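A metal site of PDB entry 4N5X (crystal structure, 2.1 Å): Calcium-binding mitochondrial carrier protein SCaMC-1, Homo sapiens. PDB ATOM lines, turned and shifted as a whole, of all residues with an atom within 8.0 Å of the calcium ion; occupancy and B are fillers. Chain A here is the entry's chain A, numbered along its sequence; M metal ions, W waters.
The side-chain amide nitrogen of Gln 45 sits close to the side-chain carboxylate of Glu 60, at 3.0 Å.
O of Gln 57 is bound to the calcium ion, 2.3 Å away. OE2 of Glu 60 is bound to the calcium ion, at 2.4 Å. OE2 of Glu 61 is bound to the calcium ion (2.4 Å). Water W1 is bound to the calcium ion. OE1 of Glu 61 is bound to the calcium ion, at 2.7 Å.
Merely in contact with the calcium ion: Gln 45 (3.98 Å). Of the 10 residues printed, 4 come within 4 Å of the calcium ion.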
ATOM      1  N   ILE A  41     -31.494 -14.779  25.482  1.00  0.00           N
ATOM      2  CA  ILE A  41     -30.470 -13.744  25.594  1.00  0.00           C
ATOM      3  C   ILE A  41     -29.081 -14.358  25.678  1.00  0.00           C
ATOM      4  O   ILE A  41     -28.096 -13.765  25.214  1.00  0.00           O
ATOM      5  CB  ILE A  41     -30.758 -12.770  26.766  1.00  0.00           C
ATOM      6  CG1 ILE A  41     -29.956 -11.477  26.597  1.00  0.00           C
ATOM      7  CG2 ILE A  41     -30.550 -13.445  28.137  1.00  0.00           C
ATOM      8  CD1 ILE A  41     -30.293 -10.407  27.608  1.00  0.00           C
ATOM      9  N   GLN A  45     -26.032 -13.820  23.246  1.00  0.00           N
ATOM     10  CA  GLN A  45     -24.733 -13.490  23.823  1.00  0.00           C
ATOM     11  C   GLN A  45     -23.617 -14.298  23.185  1.00  0.00           C
ATOM     12  O   GLN A  45     -22.601 -13.743  22.787  1.00  0.00           O
ATOM     13  CB  GLN A  45     -24.737 -13.713  25.334  1.00  0.00           C
ATOM     14  CG  GLN A  45     -23.388 -13.422  25.996  1.00  0.00           C
ATOM     15  CD  GLN A  45     -23.373 -13.841  27.452  1.00  0.00           C
ATOM     16  OE1 GLN A  45     -22.577 -14.690  27.860  1.00  0.00           O
ATOM     17  NE2 GLN A  45     -24.272 -13.263  28.254  1.00  0.00           N
ATOM     18  N   LEU A  48     -22.858 -13.104  19.528  1.00  0.00           N
ATOM     19  CA  LEU A  48     -22.068 -11.876  19.505  1.00  0.00           C
ATOM     20  C   LEU A  48     -20.601 -12.180  19.714  1.00  0.00           C
ATOM     21  O   LEU A  48     -19.714 -11.548  19.128  1.00  0.00           O
ATOM     22  CB  LEU A  48     -22.545 -10.923  20.613  1.00  0.00           C
ATOM     23  CG  LEU A  48     -23.555  -9.832  20.231  1.00  0.00           C
ATOM     24  CD1 LEU A  48     -24.481 -10.304  19.123  1.00  0.00           C
ATOM     25  CD2 LEU A  48     -24.370  -9.434  21.459  1.00  0.00           C
ATOM     26  N   GLY A  56     -19.890  -4.134  23.980  1.00  0.00           N
ATOM     27  CA  GLY A  56     -20.006  -4.128  25.430  1.00  0.00           C
ATOM     28  C   GLY A  56     -20.710  -5.389  25.901  1.00  0.00           C
ATOM     29  O   GLY A  56     -21.413  -6.049  25.137  1.00  0.00           O
ATOM     30  N   GLN A  57     -20.545  -5.732  27.165  1.00  0.00           N
ATOM     31  CA  GLN A  57     -21.213  -6.921  27.703  1.00  0.00           C
ATOM     32  C   GLN A  57     -22.726  -6.695  27.937  1.00  0.00           C
ATOM     33  O   GLN A  57     -23.405  -7.591  28.434  1.00  0.00           O
ATOM     34  CB  GLN A  57     -20.522  -7.414  28.997  1.00  0.00           C
ATOM     35  CG  GLN A  57     -19.092  -7.865  28.790  1.00  0.00           C
ATOM     36  CD  GLN A  57     -18.129  -6.697  28.656  1.00  0.00           C
ATOM     37  OE1 GLN A  57     -18.136  -5.793  29.496  1.00  0.00           O
ATOM     38  NE2 GLN A  57     -17.302  -6.706  27.618  1.00  0.00           N
ATOM     39  N   ASP A  58     -23.238  -5.520  27.566  1.00  0.00           N
ATOM     40  CA  ASP A  58     -24.672  -5.236  27.621  1.00  0.00           C
ATOM     41  C   ASP A  58     -25.304  -5.149  26.220  1.00  0.00           C
ATOM     42  O   ASP A  58     -26.407  -4.618  26.031  1.00  0.00           O
ATOM     43  CB  ASP A  58     -24.950  -3.947  28.392  1.00  0.00           C
ATOM     44  CG  ASP A  58     -24.330  -2.722  27.734  1.00  0.00           C
ATOM     45  OD1 ASP A  58     -23.446  -2.874  26.870  1.00  0.00           O
ATOM     46  OD2 ASP A  58     -24.743  -1.598  28.095  1.00  0.00           O
ATOM     47  N   ALA A  59     -24.594  -5.675  25.225  1.00  0.00           N
ATOM     48  CA  ALA A  59     -25.040  -5.540  23.851  1.00  0.00           C
ATOM     49  C   ALA A  59     -26.296  -6.380  23.573  1.00  0.00           C
ATOM     50  O   ALA A  59     -27.252  -5.892  22.985  1.00  0.00           O
ATOM     51  CB  ALA A  59     -23.907  -5.856  22.875  1.00  0.00           C
ATOM     52  N   GLU A  60     -26.297  -7.632  24.017  1.00  0.00           N
ATOM     53  CA  GLU A  60     -27.490  -8.474  23.861  1.00  0.00           C
ATOM     54  C   GLU A  60     -28.678  -7.944  24.695  1.00  0.00           C
ATOM     55  O   GLU A  60     -29.838  -8.056  24.295  1.00  0.00           O
ATOM     56  CB  GLU A  60     -27.194  -9.933  24.188  1.00  0.00           C
ATOM     57  CG  GLU A  60     -26.842 -10.230  25.640  1.00  0.00           C
ATOM     58  CD  GLU A  60     -25.355 -10.129  25.934  1.00  0.00           C
ATOM     59  OE1 GLU A  60     -24.606  -9.574  25.103  1.00  0.00           O
ATOM     60  OE2 GLU A  60     -24.938 -10.617  27.017  1.00  0.00           O
ATOM     61  N   GLU A  61     -28.383  -7.370  25.856  1.00  0.00           N
ATOM     62  CA  GLU A  61     -29.412  -6.685  26.645  1.00  0.00           C
ATOM     63  C   GLU A  61     -30.052  -5.510  25.899  1.00  0.00           C
ATOM     64  O   GLU A  61     -31.270  -5.304  25.948  1.00  0.00           O
ATOM     65  CB  GLU A  61     -28.830  -6.193  27.980  1.00  0.00           C
ATOM     66  CG  GLU A  61     -28.598  -7.293  29.013  1.00  0.00           C
ATOM     67  CD  GLU A  61     -27.237  -7.966  28.887  1.00  0.00           C
ATOM     68  OE1 GLU A  61     -26.514  -7.698  27.909  1.00  0.00           O
ATOM     69  OE2 GLU A  61     -26.880  -8.771  29.775  1.00  0.00           O
ATOM     70  N   LYS A  62     -29.227  -4.730  25.212  1.00  0.00           N
ATOM     71  CA  LYS A  62     -29.731  -3.588  24.444  1.00  0.00           C
ATOM     72  C   LYS A  62     -30.587  -4.079  23.288  1.00  0.00           C
ATOM     73  O   LYS A  62     -31.652  -3.533  23.014  1.00  0.00           O
ATOM     74  CB  LYS A  62     -28.571  -2.721  23.917  1.00  0.00           C
ATOM     75  CG  LYS A  62     -27.994  -1.772  24.967  1.00  0.00           C
ATOM     76  CD  LYS A  62     -26.768  -1.024  24.450  1.00  0.00           C
ATOM     77  CE  LYS A  62     -26.390   0.089  25.422  1.00  0.00           C
ATOM     78  NZ  LYS A  62     -25.042   0.629  25.123  1.00  0.00           N
HETATM   79 CA    CA M   1     -24.657  -9.381  29.024  1.00  0.00          CA
HETATM   80  O   HOH W   1     -24.250  -8.555  31.369  1.00  0.00           O
